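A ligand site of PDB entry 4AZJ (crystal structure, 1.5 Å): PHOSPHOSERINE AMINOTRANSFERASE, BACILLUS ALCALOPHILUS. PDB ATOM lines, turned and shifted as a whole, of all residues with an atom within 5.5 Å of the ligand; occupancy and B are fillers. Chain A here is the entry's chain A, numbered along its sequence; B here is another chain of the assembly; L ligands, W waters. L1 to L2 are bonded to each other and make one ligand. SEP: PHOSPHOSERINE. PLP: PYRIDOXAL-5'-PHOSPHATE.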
ATOM      1  N   ALA A   9      19.101  -8.972  12.781  1.00  0.00           N
ATOM      2  CA  ALA A   9      18.957  -8.940  14.237  1.00  0.00           C
ATOM      3  C   ALA A   9      19.183  -7.563  14.862  1.00  0.00           C
ATOM      4  O   ALA A   9      19.001  -7.435  16.049  1.00  0.00           O
ATOM      5  CB  ALA A   9      19.899  -9.930  14.852  1.00  0.00           C
ATOM      6  N   GLY A  10      19.591  -6.600  14.055  1.00  0.00           N
ATOM      7  CA  GLY A  10      19.864  -5.249  14.547  1.00  0.00           C
ATOM      8  C   GLY A  10      21.205  -4.758  14.088  1.00  0.00           C
ATOM      9  O   GLY A  10      22.202  -5.404  14.341  1.00  0.00           O
ATOM     10  N   GLY A  74      26.019   5.433  22.373  1.00  0.00           N
ATOM     11  CA  GLY A  74      26.883   4.393  22.928  1.00  0.00           C
ATOM     12  C   GLY A  74      26.321   3.008  22.915  1.00  0.00           C
ATOM     13  O   GLY A  74      27.009   2.066  23.252  1.00  0.00           O
ATOM     14  N   GLY A  75      25.065   2.887  22.532  1.00  0.00           N
ATOM     15  CA  GLY A  75      24.409   1.598  22.488  1.00  0.00           C
ATOM     16  C   GLY A  75      23.978   1.104  23.821  1.00  0.00           C
ATOM     17  O   GLY A  75      24.289   1.659  24.904  1.00  0.00           O
ATOM     18  N   ALA A  76      23.244  -0.013  23.808  1.00  0.00           N
ATOM     19  CA  ALA A  76      22.985  -0.690  25.067  1.00  0.00           C
ATOM     20  C   ALA A  76      24.279  -1.060  25.767  1.00  0.00           C
ATOM     21  O   ALA A  76      24.361  -1.077  27.002  1.00  0.00           O
ATOM     22  CB  ALA A  76      22.139  -1.920  24.816  1.00  0.00           C
ATOM     23  N   SER A  77      25.342  -1.353  25.021  1.00  0.00           N
ATOM     24  CA  SER A  77      26.616  -1.724  25.641  1.00  0.00           C
ATOM     25  C   SER A  77      27.121  -0.652  26.587  1.00  0.00           C
ATOM     26  O   SER A  77      27.687  -0.987  27.626  1.00  0.00           O
ATOM     27  CB  SER A  77      27.678  -2.059  24.597  1.00  0.00           C
ATOM     28  OG  SER A  77      27.252  -3.171  23.814  1.00  0.00           O
ATOM     29  N   LEU A  78      26.968   0.621  26.252  1.00  0.00           N
ATOM     30  CA  LEU A  78      27.476   1.646  27.184  1.00  0.00           C
ATOM     31  C   LEU A  78      26.620   1.649  28.435  1.00  0.00           C
ATOM     32  O   LEU A  78      27.124   1.944  29.517  1.00  0.00           O
ATOM     33  CB  LEU A  78      27.532   3.005  26.550  1.00  0.00           C
ATOM     34  CG  LEU A  78      28.246   4.089  27.379  1.00  0.00           C
ATOM     35  CD1 LEU A  78      29.696   3.764  27.594  1.00  0.00           C
ATOM     36  CD2 LEU A  78      28.112   5.419  26.680  1.00  0.00           C
ATOM     37  N   PHE A  80      25.562  -0.873  29.941  1.00  0.00           N
ATOM     38  CA  PHE A  80      26.044  -1.944  30.823  1.00  0.00           C
ATOM     39  C   PHE A  80      26.983  -1.369  31.892  1.00  0.00           C
ATOM     40  O   PHE A  80      27.039  -1.868  33.003  1.00  0.00           O
ATOM     41  CB  PHE A  80      26.787  -3.004  30.058  1.00  0.00           C
ATOM     42  CG  PHE A  80      25.946  -3.827  29.069  1.00  0.00           C
ATOM     43  CD1 PHE A  80      24.583  -3.894  29.188  1.00  0.00           C
ATOM     44  CD2 PHE A  80      26.561  -4.536  28.078  1.00  0.00           C
ATOM     45  CE1 PHE A  80      23.825  -4.670  28.313  1.00  0.00           C
ATOM     46  CE2 PHE A  80      25.780  -5.300  27.176  1.00  0.00           C
ATOM     47  CZ  PHE A  80      24.426  -5.353  27.337  1.00  0.00           C
ATOM     48  N   TRP A 102      23.666 -11.536  26.515  1.00  0.00           N
ATOM     49  CA  TRP A 102      23.540 -10.117  26.840  1.00  0.00           C
ATOM     50  C   TRP A 102      23.458  -9.905  28.346  1.00  0.00           C
ATOM     51  O   TRP A 102      24.023  -8.927  28.845  1.00  0.00           O
ATOM     52  CB  TRP A 102      22.387  -9.458  26.068  1.00  0.00           C
ATOM     53  CG  TRP A 102      22.730  -9.434  24.573  1.00  0.00           C
ATOM     54  CD1 TRP A 102      22.074 -10.062  23.567  1.00  0.00           C
ATOM     55  CD2 TRP A 102      23.874  -8.802  23.972  1.00  0.00           C
ATOM     56  NE1 TRP A 102      22.729  -9.860  22.379  1.00  0.00           N
ATOM     57  CE2 TRP A 102      23.833  -9.078  22.606  1.00  0.00           C
ATOM     58  CE3 TRP A 102      24.890  -7.998  24.478  1.00  0.00           C
ATOM     59  CZ2 TRP A 102      24.804  -8.588  21.723  1.00  0.00           C
ATOM     60  CZ3 TRP A 102      25.844  -7.514  23.618  1.00  0.00           C
ATOM     61  CH2 TRP A 102      25.816  -7.823  22.242  1.00  0.00           C
ATOM     62  N   THR A 148      17.224  -9.047  31.564  1.00  0.00           N
ATOM     63  CA  THR A 148      17.264  -8.863  30.125  1.00  0.00           C
ATOM     64  C   THR A 148      15.923  -9.387  29.608  1.00  0.00           C
ATOM     65  O   THR A 148      15.672 -10.606  29.683  1.00  0.00           O
ATOM     66  CB  THR A 148      18.411  -9.646  29.493  1.00  0.00           C
ATOM     67  OG1 THR A 148      19.626  -9.322  30.147  1.00  0.00           O
ATOM     68  CG2 THR A 148      18.565  -9.296  28.027  1.00  0.00           C
ATOM     69  N   ASN A 150      14.405  -9.737  26.717  1.00  0.00           N
ATOM     70  CA  ASN A 150      14.444 -10.582  25.547  1.00  0.00           C
ATOM     71  C   ASN A 150      15.896 -10.895  25.273  1.00  0.00           C
ATOM     72  O   ASN A 150      16.745 -10.003  25.076  1.00  0.00           O
ATOM     73  CB  ASN A 150      13.760  -9.895  24.360  1.00  0.00           C
ATOM     74  CG  ASN A 150      13.591 -10.824  23.183  1.00  0.00           C
ATOM     75  OD1 ASN A 150      12.660 -11.629  23.156  1.00  0.00           O
ATOM     76  ND2 ASN A 150      14.483 -10.726  22.222  1.00  0.00           N
ATOM     77  N   THR A 152      18.337 -11.943  23.064  1.00  0.00           N
ATOM     78  CA  THR A 152      18.338 -11.872  21.608  1.00  0.00           C
ATOM     79  C   THR A 152      19.074 -13.027  20.936  1.00  0.00           C
ATOM     80  O   THR A 152      18.669 -13.471  19.862  1.00  0.00           O
ATOM     81  CB  THR A 152      19.006 -10.548  21.200  1.00  0.00           C
ATOM     82  OG1 THR A 152      18.658  -9.544  22.148  1.00  0.00           O
ATOM     83  CG2 THR A 152      18.603 -10.111  19.764  1.00  0.00           C
ATOM     84  N   ILE A 153      20.182 -13.439  21.516  1.00  0.00           N
ATOM     85  CA  ILE A 153      21.000 -14.491  20.967  1.00  0.00           C
ATOM     86  C   ILE A 153      20.415 -15.888  21.147  1.00  0.00           C
ATOM     87  O   ILE A 153      20.541 -16.717  20.227  1.00  0.00           O
ATOM     88  CB  ILE A 153      22.430 -14.398  21.543  1.00  0.00           C
ATOM     89  CG1 ILE A 153      23.112 -13.180  20.925  1.00  0.00           C
ATOM     90  CG2 ILE A 153      23.252 -15.661  21.225  1.00  0.00           C
ATOM     91  CD1 ILE A 153      24.451 -12.789  21.589  1.00  0.00           C
ATOM     92  N   ASP A 172      17.314  -4.421  30.433  1.00  0.00           N
ATOM     93  CA  ASP A 172      17.768  -4.309  29.030  1.00  0.00           C
ATOM     94  C   ASP A 172      16.665  -4.877  28.141  1.00  0.00           C
ATOM     95  O   ASP A 172      16.489  -6.096  28.057  1.00  0.00           O
ATOM     96  CB  ASP A 172      19.054  -5.112  28.867  1.00  0.00           C
ATOM     97  CG  ASP A 172      19.606  -5.109  27.442  1.00  0.00           C
ATOM     98  OD1 ASP A 172      18.964  -4.520  26.540  1.00  0.00           O
ATOM     99  OD2 ASP A 172      20.673  -5.722  27.259  1.00  0.00           O
ATOM    100  N   SER A 174      16.435  -4.042  24.879  1.00  0.00           N
ATOM    101  CA  SER A 174      16.841  -3.723  23.515  1.00  0.00           C
ATOM    102  C   SER A 174      16.026  -4.452  22.438  1.00  0.00           C
ATOM    103  O   SER A 174      15.641  -3.837  21.472  1.00  0.00           O
ATOM    104  CB  SER A 174      18.308  -4.066  23.292  1.00  0.00           C
ATOM    105  OG  SER A 174      19.159  -3.274  24.091  1.00  0.00           O
ATOM    106  N   SER A 175      15.821  -5.756  22.600  1.00  0.00           N
ATOM    107  CA  SER A 175      15.251  -6.502  21.500  1.00  0.00           C
ATOM    108  C   SER A 175      13.759  -6.760  21.623  1.00  0.00           C
ATOM    109  O   SER A 175      13.215  -7.455  20.770  1.00  0.00           O
ATOM    110  CB  SER A 175      16.077  -7.762  21.244  1.00  0.00           C
ATOM    111  OG  SER A 175      16.235  -8.547  22.414  1.00  0.00           O
ATOM    112  N   GLY A 193      18.953  -0.234  22.949  1.00  0.00           N
ATOM    113  CA  GLY A 193      19.478   0.278  21.691  1.00  0.00           C
ATOM    114  C   GLY A 193      18.303   0.402  20.734  1.00  0.00           C
ATOM    115  O   GLY A 193      17.457  -0.478  20.695  1.00  0.00           O
ATOM    116  N   GLN A 195      18.088   0.122  17.529  1.00  0.00           N
ATOM    117  CA  GLN A 195      18.190  -0.511  16.221  1.00  0.00           C
ATOM    118  C   GLN A 195      17.524  -1.873  16.101  1.00  0.00           C
ATOM    119  O   GLN A 195      17.636  -2.502  15.057  1.00  0.00           O
ATOM    120  CB  GLN A 195      19.647  -0.623  15.828  1.00  0.00           C
ATOM    121  CG  GLN A 195      20.524  -1.564  16.643  1.00  0.00           C
ATOM    122  CD  GLN A 195      21.135  -0.963  17.885  1.00  0.00           C
ATOM    123  OE1 GLN A 195      20.818   0.151  18.280  1.00  0.00           O
ATOM    124  NE2 GLN A 195      22.056  -1.693  18.482  1.00  0.00           N
ATOM    125  N   LYS A 196      16.818  -2.342  17.115  1.00  0.00           N
ATOM    126  CA  LYS A 196      15.965  -3.541  16.890  1.00  0.00           C
ATOM    127  C   LYS A 196      14.537  -3.188  16.560  1.00  0.00           C
ATOM    128  O   LYS A 196      14.010  -3.598  15.517  1.00  0.00           O
ATOM    129  CB  LYS A 196      15.971  -4.441  18.116  1.00  0.00           C
ATOM    130  CG  LYS A 196      17.190  -5.236  18.270  1.00  0.00           C
ATOM    131  CD  LYS A 196      18.296  -4.528  18.933  1.00  0.00           C
ATOM    132  CE  LYS A 196      19.438  -5.476  19.128  1.00  0.00           C
ATOM    133  NZ  LYS A 196      20.583  -4.661  19.545  1.00  0.00           N
ATOM    134  N   THR A 204      20.290   5.259  21.834  1.00  0.00           N
ATOM    135  CA  THR A 204      19.841   4.357  22.865  1.00  0.00           C
ATOM    136  C   THR A 204      18.767   5.076  23.677  1.00  0.00           C
ATOM    137  O   THR A 204      18.955   6.245  24.089  1.00  0.00           O
ATOM    138  CB  THR A 204      21.021   3.974  23.746  1.00  0.00           C
ATOM    139  OG1 THR A 204      22.003   3.373  22.900  1.00  0.00           O
ATOM    140  CG2 THR A 204      20.638   3.014  24.837  1.00  0.00           C
ATOM    141  N   HIS A 327      23.520 -15.800  15.617  1.00  0.00           N
ATOM    142  CA  HIS A 327      24.635 -15.004  16.104  1.00  0.00           C
ATOM    143  C   HIS A 327      25.877 -15.865  16.059  1.00  0.00           C
ATOM    144  O   HIS A 327      25.833 -17.044  16.438  1.00  0.00           O
ATOM    145  CB  HIS A 327      24.349 -14.515  17.506  1.00  0.00           C
ATOM    146  CG  HIS A 327      25.326 -13.505  18.015  1.00  0.00           C
ATOM    147  ND1 HIS A 327      26.491 -13.876  18.656  1.00  0.00           N
ATOM    148  CD2 HIS A 327      25.316 -12.145  17.997  1.00  0.00           C
ATOM    149  CE1 HIS A 327      27.158 -12.791  19.017  1.00  0.00           C
ATOM    150  NE2 HIS A 327      26.467 -11.725  18.627  1.00  0.00           N
ATOM    151  N   ARG A 328      26.984 -15.271  15.628  1.00  0.00           N
ATOM    152  CA  ARG A 328      28.257 -15.999  15.444  1.00  0.00           C
ATOM    153  C   ARG A 328      28.684 -16.748  16.697  1.00  0.00           C
ATOM    154  O   ARG A 328      29.408 -17.744  16.601  1.00  0.00           O
ATOM    155  CB  ARG A 328      29.366 -15.026  15.030  1.00  0.00           C
ATOM    156  CG  ARG A 328      29.638 -13.920  16.029  1.00  0.00           C
ATOM    157  CD  ARG A 328      30.347 -12.735  15.391  1.00  0.00           C
ATOM    158  NE  ARG A 328      30.485 -11.654  16.348  1.00  0.00           N
ATOM    159  CZ  ARG A 328      29.506 -10.813  16.679  1.00  0.00           C
ATOM    160  NH1 ARG A 328      28.324 -10.893  16.109  1.00  0.00           N
ATOM    161  NH2 ARG A 328      29.722  -9.904  17.605  1.00  0.00           N
ATOM    162  N   ARG A 334      18.654 -17.862  13.265  1.00  0.00           N
ATOM    163  CA  ARG A 334      17.869 -16.945  14.060  1.00  0.00           C
ATOM    164  C   ARG A 334      17.058 -16.095  13.113  1.00  0.00           C
ATOM    165  O   ARG A 334      17.596 -15.338  12.312  1.00  0.00           O
ATOM    166  CB  ARG A 334      18.792 -16.087  14.944  1.00  0.00           C
ATOM    167  CG  ARG A 334      18.056 -15.043  15.760  1.00  0.00           C
ATOM    168  CD  ARG A 334      18.939 -14.282  16.742  1.00  0.00           C
ATOM    169  NE  ARG A 334      20.053 -13.622  16.101  1.00  0.00           N
ATOM    170  CZ  ARG A 334      20.892 -12.787  16.726  1.00  0.00           C
ATOM    171  NH1 ARG A 334      20.696 -12.505  18.012  1.00  0.00           N
ATOM    172  NH2 ARG A 334      21.918 -12.276  16.056  1.00  0.00           N
ATOM    173  N   HIS B  41      25.414  -4.654  10.862  1.00  0.00           N
ATOM    174  CA  HIS B  41      26.828  -4.334  10.952  1.00  0.00           C
ATOM    175  C   HIS B  41      27.744  -5.513  10.826  1.00  0.00           C
ATOM    176  O   HIS B  41      28.936  -5.334  10.656  1.00  0.00           O
ATOM    177  CB  HIS B  41      27.133  -3.603  12.258  1.00  0.00           C
ATOM    178  CG  HIS B  41      26.716  -4.343  13.484  1.00  0.00           C
ATOM    179  ND1 HIS B  41      25.430  -4.793  13.674  1.00  0.00           N
ATOM    180  CD2 HIS B  41      27.395  -4.681  14.605  1.00  0.00           C
ATOM    181  CE1 HIS B  41      25.332  -5.378  14.846  1.00  0.00           C
ATOM    182  NE2 HIS B  41      26.519  -5.324  15.436  1.00  0.00           N
ATOM    183  N   ARG B  42      27.171  -6.728  10.863  1.00  0.00           N
ATOM    184  CA  ARG B  42      27.920  -7.984  10.660  1.00  0.00           C
ATOM    185  C   ARG B  42      27.868  -8.461   9.210  1.00  0.00           C
ATOM    186  O   ARG B  42      28.377  -9.550   8.911  1.00  0.00           O
ATOM    187  CB  ARG B  42      27.403  -9.063  11.625  1.00  0.00           C
ATOM    188  CG  ARG B  42      27.328  -8.627  13.084  1.00  0.00           C
ATOM    189  CD  ARG B  42      28.715  -8.317  13.642  1.00  0.00           C
ATOM    190  NE  ARG B  42      28.671  -7.762  14.997  1.00  0.00           N
ATOM    191  CZ  ARG B  42      29.669  -7.112  15.559  1.00  0.00           C
ATOM    192  NH1 ARG B  42      30.815  -6.933  14.922  1.00  0.00           N
ATOM    193  NH2 ARG B  42      29.489  -6.593  16.765  1.00  0.00           N
ATOM    194  N   TYR B 236      33.030  -3.474  17.757  1.00  0.00           N
ATOM    195  CA  TYR B 236      32.842  -4.200  18.982  1.00  0.00           C
ATOM    196  C   TYR B 236      31.369  -4.328  19.306  1.00  0.00           C
ATOM    197  O   TYR B 236      30.860  -5.414  19.570  1.00  0.00           O
ATOM    198  CB  TYR B 236      33.562  -3.523  20.172  1.00  0.00           C
ATOM    199  CG  TYR B 236      33.201  -4.208  21.460  1.00  0.00           C
ATOM    200  CD1 TYR B 236      33.699  -5.471  21.752  1.00  0.00           C
ATOM    201  CD2 TYR B 236      32.340  -3.620  22.360  1.00  0.00           C
ATOM    202  CE1 TYR B 236      33.338  -6.094  22.933  1.00  0.00           C
ATOM    203  CE2 TYR B 236      31.990  -4.235  23.538  1.00  0.00           C
ATOM    204  CZ  TYR B 236      32.500  -5.468  23.824  1.00  0.00           C
ATOM    205  OH  TYR B 236      32.146  -6.108  24.981  1.00  0.00           O
ATOM    206  N   ASN B 237      30.688  -3.181  19.329  1.00  0.00           N
ATOM    207  CA  ASN B 237      29.238  -3.155  19.432  1.00  0.00           C
ATOM    208  C   ASN B 237      28.669  -2.536  18.161  1.00  0.00           C
ATOM    209  O   ASN B 237      29.383  -2.359  17.171  1.00  0.00           O
ATOM    210  CB  ASN B 237      28.730  -2.471  20.710  1.00  0.00           C
ATOM    211  CG  ASN B 237      28.863  -0.974  20.667  1.00  0.00           C
ATOM    212  OD1 ASN B 237      29.818  -0.448  20.069  1.00  0.00           O
ATOM    213  ND2 ASN B 237      27.885  -0.284  21.247  1.00  0.00           N
ATOM    214  N   THR B 238      27.373  -2.275  18.135  1.00  0.00           N
ATOM    215  CA  THR B 238      26.730  -1.829  16.894  1.00  0.00           C
ATOM    216  C   THR B 238      27.145  -0.376  16.617  1.00  0.00           C
ATOM    217  O   THR B 238      26.881   0.501  17.439  1.00  0.00           O
ATOM    218  CB  THR B 238      25.213  -1.920  17.002  1.00  0.00           C
ATOM    219  OG1 THR B 238      24.853  -3.209  17.466  1.00  0.00           O
ATOM    220  CG2 THR B 238      24.610  -1.674  15.640  1.00  0.00           C
HETATM  221  N   SEP L   1      22.257  -7.566  19.901  1.00  0.00           N
HETATM  222  CA  SEP L   1      22.574  -7.920  18.547  1.00  0.00           C
HETATM  223  CB  SEP L   1      23.927  -7.435  18.046  1.00  0.00           C
HETATM  224  OG  SEP L   1      24.987  -8.273  18.506  1.00  0.00           O
HETATM  225  C   SEP L   1      22.402  -9.407  18.320  1.00  0.00           C
HETATM  226  O   SEP L   1      22.652  -9.819  17.168  1.00  0.00           O
HETATM  227  OXT SEP L   1      22.012 -10.134  19.264  1.00  0.00           O
HETATM  228  P   SEP L   1      26.442  -8.178  17.911  1.00  0.00           P
HETATM  229  O1P SEP L   1      26.405  -8.658  16.479  1.00  0.00           O
HETATM  230  O2P SEP L   1      26.855  -6.701  17.943  1.00  0.00           O
HETATM  231  O3P SEP L   1      27.242  -9.079  18.816  1.00  0.00           O
HETATM  232  N1  PLP L   2      21.428  -6.044  24.632  1.00  0.00           N
HETATM  233  C2  PLP L   2      20.660  -6.790  23.834  1.00  0.00           C
HETATM  234  C2A PLP L   2      19.483  -7.502  24.433  1.00  0.00           C
HETATM  235  C3  PLP L   2      21.015  -6.912  22.436  1.00  0.00           C
HETATM  236  O3  PLP L   2      20.252  -7.661  21.654  1.00  0.00           O
HETATM  237  C4  PLP L   2      22.164  -6.190  21.898  1.00  0.00           C
HETATM  238  C4A PLP L   2      22.582  -6.380  20.490  1.00  0.00           C
HETATM  239  C5  PLP L   2      22.883  -5.413  22.799  1.00  0.00           C
HETATM  240  C6  PLP L   2      22.493  -5.366  24.130  1.00  0.00           C
HETATM  241  C5A PLP L   2      24.095  -4.615  22.375  1.00  0.00           C
HETATM  242  O4P PLP L   2      23.618  -3.387  21.747  1.00  0.00           O
HETATM  243  P   PLP L   2      24.659  -2.311  21.137  1.00  0.00           P
HETATM  244  O1P PLP L   2      23.764  -1.199  20.699  1.00  0.00           O
HETATM  245  O2P PLP L   2      25.347  -3.027  20.031  1.00  0.00           O
HETATM  246  O3P PLP L   2      25.631  -1.938  22.261  1.00  0.00           O
HETATM  247  O   HOH W   1      22.395  -4.511  17.107  1.00  0.00           O
HETATM  248  O   HOH W   2      24.242  -9.259  15.107  1.00  0.00           O
HETATM  249  O   HOH W   3      26.930  -5.348  20.229  1.00  0.00           O
HETATM  250  O   HOH W   4      25.028   0.865  19.428  1.00  0.00           O
HETATM  251  O   HOH W   5      20.794  -2.738  21.755  1.00  0.00           O
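NH1 of Arg 334 sits at hydrogen-bond distance from O of Thr 152 (2.9 Å).
The side-chain hydroxyl of Thr 152 is in hydrogen-bond range of the side-chain hydroxyl of Ser 175 (2.6 Å).
The guanidinium group of Arg 328 lies within hydrogen-bond range of a ring nitrogen (NE2) of His 327 (3.2 Å).
The side-chain amino group of Lys 196 sits close to the side-chain amide nitrogen of Gln 195 (3.5 Å).
The guanidinium group (NE) of Arg 42 of chain B lies within hydrogen-bond range of a ring nitrogen (NE2) of His 41 of chain B (3.3 Å).
The side-chain amide nitrogen (ND2) of Asn 237 of chain B is in hydrogen-bond range of the backbone carbonyl oxygen (O) of Gly 74, 3.2 Å away.
N of Gly 193 lies within hydrogen-bond range of OG of Ser 174, 3.3 Å away.
OG of Ser 175 is in hydrogen-bond range of ND2 of Asn 150 (2.8 Å).
Water W4 bridges O1P of PLP L2 and O of Thr 238 of chain B.
Water W5 lies within hydrogen-bond range of an oxygen (O4P) of PLP L2 (2.9 Å), the side-chain hydroxyl (OG) of Ser 174 (2.9 Å), the side-chain amino group (NZ) of Lys 196 (2.9 Å) and the backbone NH (N) of Gly 193 (3.3 Å).
Water W1 lies within hydrogen-bond range of the side-chain hydroxyl of Thr 238 of chain B (2.8 Å), the backbone carbonyl oxygen of Gly 10 (2.9 Å), the side-chain amino group of Lys 196 (3.0 Å) and the side-chain amide nitrogen of Gln 195 (3.2 Å).
Merely in contact with the ligand: Gly 75, Ala 9, Ser 174, Ile 153, Phe 80, Asn 150 and Ser 175.
Hydrophobic or aromatic side chains within 4 Å of the ligand: Ala 9, Ala 76, Phe 80, Trp 102, Ile 153, His 327 and His 41 of chain B.
Of the 28 residues printed, 21 come within 4 Å of the ligand.
Along chain A the residues within 4 Å of the ligand span positions 9 to 334.
O3 of PLP L2 lies within hydrogen-bond range of OG1 of Thr 152.
The backbone NH (N) of Ser 77 is in hydrogen-bond range of an oxygen (O3P) of PLP L2 (2.8 Å).
OG of Ser 77 is in hydrogen-bond range of O3P of PLP L2 (2.6 Å).
The backbone NH (N) of Thr 238 of chain B lies within hydrogen-bond range of an oxygen (O2P) of PLP L2 (2.9 Å).
OG1 of Thr 238 of chain B lies within hydrogen-bond range of O2P of PLP L2, at 2.6 Å.
OD2 of Asp 172 is in hydrogen-bond range of N1 of PLP L2 (2.8 Å).
NE2 of His 327 sits at hydrogen-bond distance from O3P of SEP L1, 2.8 Å away.
The guanidinium group (NH2) of Arg 334 is in salt-bridge range of an oxygen (O) of SEP L1.
N of SEP L1 sits close to NZ of Lys 196.
O1P of PLP L2 is in hydrogen-bond range of NE2 of Gln 195 (2.8 Å).
The guanidinium group (NE) of Arg 42 of chain B lies within salt-bridge range of an oxygen (O1P) of SEP L1.
The guanidinium group (NH2) of Arg 328 lies within salt-bridge range of an oxygen (O3P) of SEP L1, at 2.9 Å.
NE2 of His 41 of chain B lies within hydrogen-bond range of O2P of SEP L1, at 2.9 Å.
ND2 of Asn 237 of chain B is in hydrogen-bond range of O3P of PLP L2 (3.0 Å).
An oxygen (OXT) of SEP L1 lies within hydrogen-bond range of the indole nitrogen (NE1) of Trp 102, at 3.2 Å.
N of Ala 76 is in hydrogen-bond range of O1P of PLP L2, 3.4 Å away.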
